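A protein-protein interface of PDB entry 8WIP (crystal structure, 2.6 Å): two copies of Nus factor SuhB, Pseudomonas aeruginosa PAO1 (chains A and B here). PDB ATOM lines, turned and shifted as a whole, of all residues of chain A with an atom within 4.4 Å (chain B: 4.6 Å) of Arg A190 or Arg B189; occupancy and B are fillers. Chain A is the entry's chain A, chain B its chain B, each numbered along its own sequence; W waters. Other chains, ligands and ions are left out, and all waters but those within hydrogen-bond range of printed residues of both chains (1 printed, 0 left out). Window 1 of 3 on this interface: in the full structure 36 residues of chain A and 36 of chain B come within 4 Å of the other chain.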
ATOM      1  N   ASN A  95       0.469  27.790 -35.334  1.00  0.00           N
ATOM      2  CA  ASN A  95      -0.776  28.470 -34.969  1.00  0.00           C
ATOM      3  C   ASN A  95      -1.133  29.548 -35.983  1.00  0.00           C
ATOM      4  O   ASN A  95      -2.253  29.581 -36.506  1.00  0.00           O
ATOM      5  CB  ASN A  95      -0.634  29.126 -33.586  1.00  0.00           C
ATOM      6  CG  ASN A  95      -0.720  28.127 -32.424  1.00  0.00           C
ATOM      7  OD1 ASN A  95      -0.939  26.940 -32.617  1.00  0.00           O
ATOM      8  ND2 ASN A  95      -0.481  28.618 -31.215  1.00  0.00           N
ATOM      9  N   THR A 159       3.884  23.386 -21.686  1.00  0.00           N
ATOM     10  CA  THR A 159       4.898  22.570 -22.350  1.00  0.00           C
ATOM     11  C   THR A 159       4.701  22.656 -23.863  1.00  0.00           C
ATOM     12  O   THR A 159       3.696  23.191 -24.340  1.00  0.00           O
ATOM     13  CB  THR A 159       4.813  21.117 -21.863  1.00  0.00           C
ATOM     14  OG1 THR A 159       5.949  20.368 -22.291  1.00  0.00           O
ATOM     15  CG2 THR A 159       3.572  20.457 -22.402  1.00  0.00           C
ATOM     16  N   GLY A 160       5.710  22.196 -24.621  1.00  0.00           N
ATOM     17  CA  GLY A 160       5.504  22.008 -26.050  1.00  0.00           C
ATOM     18  C   GLY A 160       6.488  21.085 -26.760  1.00  0.00           C
ATOM     19  O   GLY A 160       7.669  21.069 -26.415  1.00  0.00           O
ATOM     20  N   PHE A 161       6.003  20.164 -27.577  1.00  0.00           N
ATOM     21  CA  PHE A 161       6.934  19.253 -28.247  1.00  0.00           C
ATOM     22  C   PHE A 161       7.541  19.874 -29.515  1.00  0.00           C
ATOM     23  O   PHE A 161       6.843  20.582 -30.244  1.00  0.00           O
ATOM     24  CB  PHE A 161       6.258  17.938 -28.587  1.00  0.00           C
ATOM     25  CG  PHE A 161       7.234  16.845 -28.914  1.00  0.00           C
ATOM     26  CD1 PHE A 161       8.074  16.326 -27.934  1.00  0.00           C
ATOM     27  CD2 PHE A 161       7.329  16.357 -30.200  1.00  0.00           C
ATOM     28  CE1 PHE A 161       8.983  15.322 -28.239  1.00  0.00           C
ATOM     29  CE2 PHE A 161       8.227  15.365 -30.513  1.00  0.00           C
ATOM     30  CZ  PHE A 161       9.061  14.846 -29.531  1.00  0.00           C
ATOM     31  N   TYR A 174      10.251  12.565 -23.813  1.00  0.00           N
ATOM     32  CA  TYR A 174       9.236  13.568 -23.525  1.00  0.00           C
ATOM     33  C   TYR A 174       8.006  12.942 -22.917  1.00  0.00           C
ATOM     34  O   TYR A 174       7.516  13.383 -21.868  1.00  0.00           O
ATOM     35  CB  TYR A 174       8.873  14.347 -24.779  1.00  0.00           C
ATOM     36  CG  TYR A 174       7.791  15.351 -24.482  1.00  0.00           C
ATOM     37  CD1 TYR A 174       8.074  16.624 -23.977  1.00  0.00           C
ATOM     38  CD2 TYR A 174       6.463  15.024 -24.743  1.00  0.00           C
ATOM     39  CE1 TYR A 174       7.050  17.531 -23.719  1.00  0.00           C
ATOM     40  CE2 TYR A 174       5.444  15.917 -24.493  1.00  0.00           C
ATOM     41  CZ  TYR A 174       5.742  17.170 -23.990  1.00  0.00           C
ATOM     42  OH  TYR A 174       4.704  18.028 -23.749  1.00  0.00           O
ATOM     43  N   PHE A 178       6.044  13.861 -19.386  1.00  0.00           N
ATOM     44  CA  PHE A 178       4.601  14.043 -19.338  1.00  0.00           C
ATOM     45  C   PHE A 178       3.964  12.986 -18.425  1.00  0.00           C
ATOM     46  O   PHE A 178       3.157  13.321 -17.545  1.00  0.00           O
ATOM     47  CB  PHE A 178       3.990  14.059 -20.745  1.00  0.00           C
ATOM     48  CG  PHE A 178       2.510  14.403 -20.786  1.00  0.00           C
ATOM     49  CD1 PHE A 178       1.570  13.424 -20.524  1.00  0.00           C
ATOM     50  CD2 PHE A 178       2.057  15.693 -21.123  1.00  0.00           C
ATOM     51  CE1 PHE A 178       0.195  13.697 -20.568  1.00  0.00           C
ATOM     52  CE2 PHE A 178       0.673  15.976 -21.168  1.00  0.00           C
ATOM     53  CZ  PHE A 178      -0.255  14.972 -20.881  1.00  0.00           C
ATOM     54  N   ILE A 188      -1.913  20.144 -17.891  1.00  0.00           N
ATOM     55  CA  ILE A 188      -0.763  20.461 -18.720  1.00  0.00           C
ATOM     56  C   ILE A 188      -1.309  21.000 -20.024  1.00  0.00           C
ATOM     57  O   ILE A 188      -2.265  20.446 -20.580  1.00  0.00           O
ATOM     58  CB  ILE A 188       0.151  19.242 -18.932  1.00  0.00           C
ATOM     59  CG1 ILE A 188       0.497  18.630 -17.567  1.00  0.00           C
ATOM     60  CG2 ILE A 188       1.413  19.664 -19.656  1.00  0.00           C
ATOM     61  CD1 ILE A 188       1.314  17.364 -17.599  1.00  0.00           C
ATOM     62  N   ARG A 189      -0.696  22.062 -20.517  1.00  0.00           N
ATOM     63  CA  ARG A 189      -1.148  22.784 -21.697  1.00  0.00           C
ATOM     64  C   ARG A 189      -0.033  22.854 -22.709  1.00  0.00           C
ATOM     65  O   ARG A 189       1.130  22.990 -22.332  1.00  0.00           O
ATOM     66  CB  ARG A 189      -1.637  24.191 -21.407  1.00  0.00           C
ATOM     67  CG  ARG A 189      -2.805  24.252 -20.457  1.00  0.00           C
ATOM     68  CD  ARG A 189      -4.118  23.754 -21.116  1.00  0.00           C
ATOM     69  NE  ARG A 189      -5.252  23.824 -20.187  1.00  0.00           N
ATOM     70  CZ  ARG A 189      -5.639  22.839 -19.390  1.00  0.00           C
ATOM     71  NH1 ARG A 189      -5.009  21.670 -19.378  1.00  0.00           N
ATOM     72  NH2 ARG A 189      -6.702  23.018 -18.608  1.00  0.00           N
ATOM     73  N   ARG A 190      -0.406  22.640 -23.974  1.00  0.00           N
ATOM     74  CA  ARG A 190       0.454  22.790 -25.150  1.00  0.00           C
ATOM     75  C   ARG A 190      -0.261  23.757 -26.089  1.00  0.00           C
ATOM     76  O   ARG A 190      -1.087  23.362 -26.910  1.00  0.00           O
ATOM     77  CB  ARG A 190       0.679  21.442 -25.841  1.00  0.00           C
ATOM     78  CG  ARG A 190       1.920  21.390 -26.762  1.00  0.00           C
ATOM     79  CD  ARG A 190       2.547  19.993 -26.997  1.00  0.00           C
ATOM     80  NE  ARG A 190       2.370  19.070 -25.875  1.00  0.00           N
ATOM     81  CZ  ARG A 190       1.478  18.089 -25.840  1.00  0.00           C
ATOM     82  NH1 ARG A 190       0.667  17.854 -26.866  1.00  0.00           N
ATOM     83  NH2 ARG A 190       1.426  17.294 -24.762  1.00  0.00           N
ATOM     84  N   ALA A 191       0.002  25.052 -25.907  1.00  0.00           N
ATOM     85  CA  ALA A 191      -0.693  26.062 -26.688  1.00  0.00           C
ATOM     86  C   ALA A 191       0.065  26.502 -27.940  1.00  0.00           C
ATOM     87  O   ALA A 191      -0.546  27.079 -28.843  1.00  0.00           O
ATOM     88  CB  ALA A 191      -0.997  27.279 -25.797  1.00  0.00           C
ATOM     89  N   GLY A 192       1.372  26.281 -28.003  1.00  0.00           N
ATOM     90  CA  GLY A 192       2.156  26.432 -29.226  1.00  0.00           C
ATOM     91  C   GLY A 192       2.958  27.716 -29.369  1.00  0.00           C
ATOM     92  O   GLY A 192       3.447  27.992 -30.468  1.00  0.00           O
ATOM     93  N   LEU B 156      -2.761  20.201 -38.078  1.00  0.00           N
ATOM     94  CA  LEU B 156      -2.776  20.682 -36.698  1.00  0.00           C
ATOM     95  C   LEU B 156      -3.998  20.087 -35.999  1.00  0.00           C
ATOM     96  O   LEU B 156      -5.129  20.315 -36.431  1.00  0.00           O
ATOM     97  CB  LEU B 156      -2.767  22.209 -36.636  1.00  0.00           C
ATOM     98  CG  LEU B 156      -2.687  22.805 -35.234  1.00  0.00           C
ATOM     99  CD1 LEU B 156      -1.357  22.481 -34.531  1.00  0.00           C
ATOM    100  CD2 LEU B 156      -2.895  24.315 -35.291  1.00  0.00           C
ATOM    101  N   LEU B 157      -3.757  19.202 -35.035  1.00  0.00           N
ATOM    102  CA  LEU B 157      -4.820  18.543 -34.287  1.00  0.00           C
ATOM    103  C   LEU B 157      -4.976  19.179 -32.896  1.00  0.00           C
ATOM    104  O   LEU B 157      -4.010  19.708 -32.334  1.00  0.00           O
ATOM    105  CB  LEU B 157      -4.479  17.057 -34.156  1.00  0.00           C
ATOM    106  CG  LEU B 157      -4.104  16.318 -35.445  1.00  0.00           C
ATOM    107  CD1 LEU B 157      -4.015  14.837 -35.208  1.00  0.00           C
ATOM    108  CD2 LEU B 157      -5.220  16.569 -36.441  1.00  0.00           C
ATOM    109  N   GLY B 158      -6.207  19.231 -32.384  1.00  0.00           N
ATOM    110  CA  GLY B 158      -6.457  19.517 -30.975  1.00  0.00           C
ATOM    111  C   GLY B 158      -6.866  18.293 -30.171  1.00  0.00           C
ATOM    112  O   GLY B 158      -7.412  17.333 -30.716  1.00  0.00           O
ATOM    113  N   THR B 159      -6.619  18.317 -28.867  1.00  0.00           N
ATOM    114  CA  THR B 159      -7.072  17.213 -28.030  1.00  0.00           C
ATOM    115  C   THR B 159      -7.055  17.680 -26.585  1.00  0.00           C
ATOM    116  O   THR B 159      -6.542  18.756 -26.286  1.00  0.00           O
ATOM    117  CB  THR B 159      -6.199  15.965 -28.225  1.00  0.00           C
ATOM    118  OG1 THR B 159      -6.808  14.837 -27.589  1.00  0.00           O
ATOM    119  CG2 THR B 159      -4.829  16.185 -27.666  1.00  0.00           C
ATOM    120  N   PHE B 178      -1.222   9.661 -29.186  1.00  0.00           N
ATOM    121  CA  PHE B 178      -0.286  10.760 -29.402  1.00  0.00           C
ATOM    122  C   PHE B 178       0.938  10.302 -30.193  1.00  0.00           C
ATOM    123  O   PHE B 178       1.331  10.950 -31.173  1.00  0.00           O
ATOM    124  CB  PHE B 178       0.115  11.377 -28.058  1.00  0.00           C
ATOM    125  CG  PHE B 178       0.941  12.641 -28.184  1.00  0.00           C
ATOM    126  CD1 PHE B 178       0.314  13.872 -28.356  1.00  0.00           C
ATOM    127  CD2 PHE B 178       2.329  12.603 -28.135  1.00  0.00           C
ATOM    128  CE1 PHE B 178       1.060  15.041 -28.487  1.00  0.00           C
ATOM    129  CE2 PHE B 178       3.086  13.777 -28.263  1.00  0.00           C
ATOM    130  CZ  PHE B 178       2.449  14.995 -28.437  1.00  0.00           C
ATOM    131  N   GLY B 187       1.559  19.656 -35.546  1.00  0.00           N
ATOM    132  CA  GLY B 187       1.408  19.910 -34.133  1.00  0.00           C
ATOM    133  C   GLY B 187       0.138  19.298 -33.574  1.00  0.00           C
ATOM    134  O   GLY B 187      -0.853  19.072 -34.286  1.00  0.00           O
ATOM    135  N   ILE B 188       0.170  19.095 -32.267  1.00  0.00           N
ATOM    136  CA  ILE B 188      -0.983  18.684 -31.481  1.00  0.00           C
ATOM    137  C   ILE B 188      -1.064  19.693 -30.351  1.00  0.00           C
ATOM    138  O   ILE B 188      -0.065  19.963 -29.670  1.00  0.00           O
ATOM    139  CB  ILE B 188      -0.882  17.233 -30.979  1.00  0.00           C
ATOM    140  CG1 ILE B 188      -0.582  16.303 -32.166  1.00  0.00           C
ATOM    141  CG2 ILE B 188      -2.173  16.826 -30.294  1.00  0.00           C
ATOM    142  CD1 ILE B 188      -0.362  14.859 -31.819  1.00  0.00           C
ATOM    143  N   ARG B 189      -2.268  20.144 -30.066  1.00  0.00           N
ATOM    144  CA  ARG B 189      -2.520  21.213 -29.113  1.00  0.00           C
ATOM    145  C   ARG B 189      -3.474  20.780 -28.023  1.00  0.00           C
ATOM    146  O   ARG B 189      -4.516  20.174 -28.284  1.00  0.00           O
ATOM    147  CB  ARG B 189      -3.085  22.461 -29.795  1.00  0.00           C
ATOM    148  CG  ARG B 189      -2.205  23.072 -30.822  1.00  0.00           C
ATOM    149  CD  ARG B 189      -1.011  23.786 -30.148  1.00  0.00           C
ATOM    150  NE  ARG B 189       0.255  23.377 -30.748  1.00  0.00           N
ATOM    151  CZ  ARG B 189       0.903  24.049 -31.691  1.00  0.00           C
ATOM    152  NH1 ARG B 189       0.431  25.185 -32.177  1.00  0.00           N
ATOM    153  NH2 ARG B 189       2.014  23.529 -32.208  1.00  0.00           N
ATOM    154  N   ARG B 190      -3.131  21.172 -26.808  1.00  0.00           N
ATOM    155  CA  ARG B 190      -3.984  20.967 -25.646  1.00  0.00           C
ATOM    156  C   ARG B 190      -4.189  22.351 -25.023  1.00  0.00           C
ATOM    157  O   ARG B 190      -3.365  22.857 -24.261  1.00  0.00           O
ATOM    158  CB  ARG B 190      -3.301  19.976 -24.680  1.00  0.00           C
ATOM    159  CG  ARG B 190      -4.206  19.254 -23.682  1.00  0.00           C
ATOM    160  CD  ARG B 190      -3.361  18.486 -22.635  1.00  0.00           C
ATOM    161  NE  ARG B 190      -2.162  17.938 -23.260  1.00  0.00           N
ATOM    162  CZ  ARG B 190      -2.148  16.751 -23.857  1.00  0.00           C
ATOM    163  NH1 ARG B 190      -3.243  16.004 -23.924  1.00  0.00           N
ATOM    164  NH2 ARG B 190      -1.027  16.321 -24.441  1.00  0.00           N
ATOM    165  N   ALA B 191      -5.234  23.044 -25.485  1.00  0.00           N
ATOM    166  CA  ALA B 191      -5.460  24.404 -25.013  1.00  0.00           C
ATOM    167  C   ALA B 191      -6.426  24.488 -23.815  1.00  0.00           C
ATOM    168  O   ALA B 191      -6.420  25.491 -23.095  1.00  0.00           O
ATOM    169  CB  ALA B 191      -5.972  25.277 -26.171  1.00  0.00           C
ATOM    170  N   TYR B 206      -8.166  24.116 -36.728  1.00  0.00           N
ATOM    171  CA  TYR B 206      -7.660  22.755 -36.558  1.00  0.00           C
ATOM    172  C   TYR B 206      -8.174  21.876 -37.686  1.00  0.00           C
ATOM    173  O   TYR B 206      -9.322  22.002 -38.125  1.00  0.00           O
ATOM    174  CB  TYR B 206      -8.143  22.072 -35.276  1.00  0.00           C
ATOM    175  CG  TYR B 206      -7.659  22.626 -33.988  1.00  0.00           C
ATOM    176  CD1 TYR B 206      -6.536  23.423 -33.911  1.00  0.00           C
ATOM    177  CD2 TYR B 206      -8.340  22.324 -32.812  1.00  0.00           C
ATOM    178  CE1 TYR B 206      -6.132  23.938 -32.680  1.00  0.00           C
ATOM    179  CE2 TYR B 206      -7.946  22.824 -31.612  1.00  0.00           C
ATOM    180  CZ  TYR B 206      -6.846  23.619 -31.542  1.00  0.00           C
ATOM    181  OH  TYR B 206      -6.481  24.102 -30.310  1.00  0.00           O
HETATM  182  O   HOH W   1       2.810  27.507 -33.246  1.00  0.00           O
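The side-chain amide oxygen (OD1) of Asn A95 sits close to the guanidinium group (NH1) of Arg B189 (2.3 Å).
The backbone NH (N) of Arg A190 lies within hydrogen-bond range of the backbone carbonyl oxygen (O) of Arg B190 (3.0 Å).
The backbone carbonyl oxygen (O) of Leu B157 lies within hydrogen-bond range of the backbone NH (N) of Arg B189 (2.9 Å).
ND2 of Asn A95 is in hydrogen-bond range of O of Ala A191.
N of Thr B159 lies within hydrogen-bond range of O of Arg B189, 2.9 Å away.
The backbone NH (N) of Thr A159 lies within hydrogen-bond range of the backbone carbonyl oxygen (O) of Arg A189, 2.9 Å away.
The side-chain hydroxyl (OH) of Tyr A174 lies within hydrogen-bond range of the guanidinium group (NE) of Arg A190 (3.3 Å).
Among the printed residues, merely in contact across the chains: Phe A178 with Arg B190 (3.7 Å), Ile A188 with Arg B190 (3.0 Å), Arg A189 with Arg B190 (3.4 Å), Arg A189 with Ala B191 (3.5 Å), Arg A190 with Phe B178 (3.3 Å), Arg A190 with Ile B188 (3.6 Å), Arg A190 with Arg B189 (3.3 Å), Ala A191 with Arg B189 (3.6 Å) and Gly A192 with Arg B189 (3.6 Å).
Of the printed residues of chain B, Asn A95 touches Arg B189.
Phe A161 touches none of the printed residues of chain B.
Printed residues of chain B within 4 Å of Phe A178: Arg B190 (3.7 Å).
Arg A190 touches just these residues of chain B: Phe B178 (3.3 Å), Ile B188 (3.6 Å), Arg B189 (3.3 Å) and Arg B190 (2.7 Å).
Printed residues of chain B within 4 Å of Ala A191: Arg B189 (3.6 Å).
Leu B157 touches none of the printed residues of chain A.
Of chain A, only Asn A95 (2.3 Å), Arg A190 (3.3 Å), Ala A191 (3.6 Å) and Gly A192 (3.6 Å) come within 4 Å of Arg B189.
Of the printed residues of chain A, Arg B190 touches Phe A178 (3.7 Å), Ile A188 (3.0 Å), Arg A189 (3.4 Å) and Arg A190 (2.7 Å).
The nearest residue of chain B that does not touch Arg A190 is Ala B191 (4.4 Å).
The nearest printed residue of chain A that does not touch Ala B191 is Arg A190 (4.4 Å).
Of the 11 printed residues of chain A, 7 touch a printed residue of chain B.
Hydrophobic or aromatic side chains of chain A that line the printed part of chain B: Phe A178.
Among the printed residues, 11 pairs touch across the chains.
Phe A178 touches Arg B190, and with the chains exchanged Arg A190 touches Phe B178.
Ile A188 touches Arg B190, and with the chains exchanged Arg A190 touches Ile B188.
Arg A189 touches Ala B191, and with the chains exchanged Ala A191 touches Arg B189.
Arg A190 touches its own counterpart, Arg B190.
Positions printed for both chains: 159, 178, 188, 189, 190 and 191.
Of the 11 pairs that touch across the chains among the printed residues, 9 have their exchanged pair printed and touching as well.
Water W1 lies within hydrogen-bond range of the backbone carbonyl oxygen of Gly A192 (2.9 Å), the backbone NH of Asn A95 (3.1 Å) and the guanidinium group of Arg B189 (3.5 Å).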
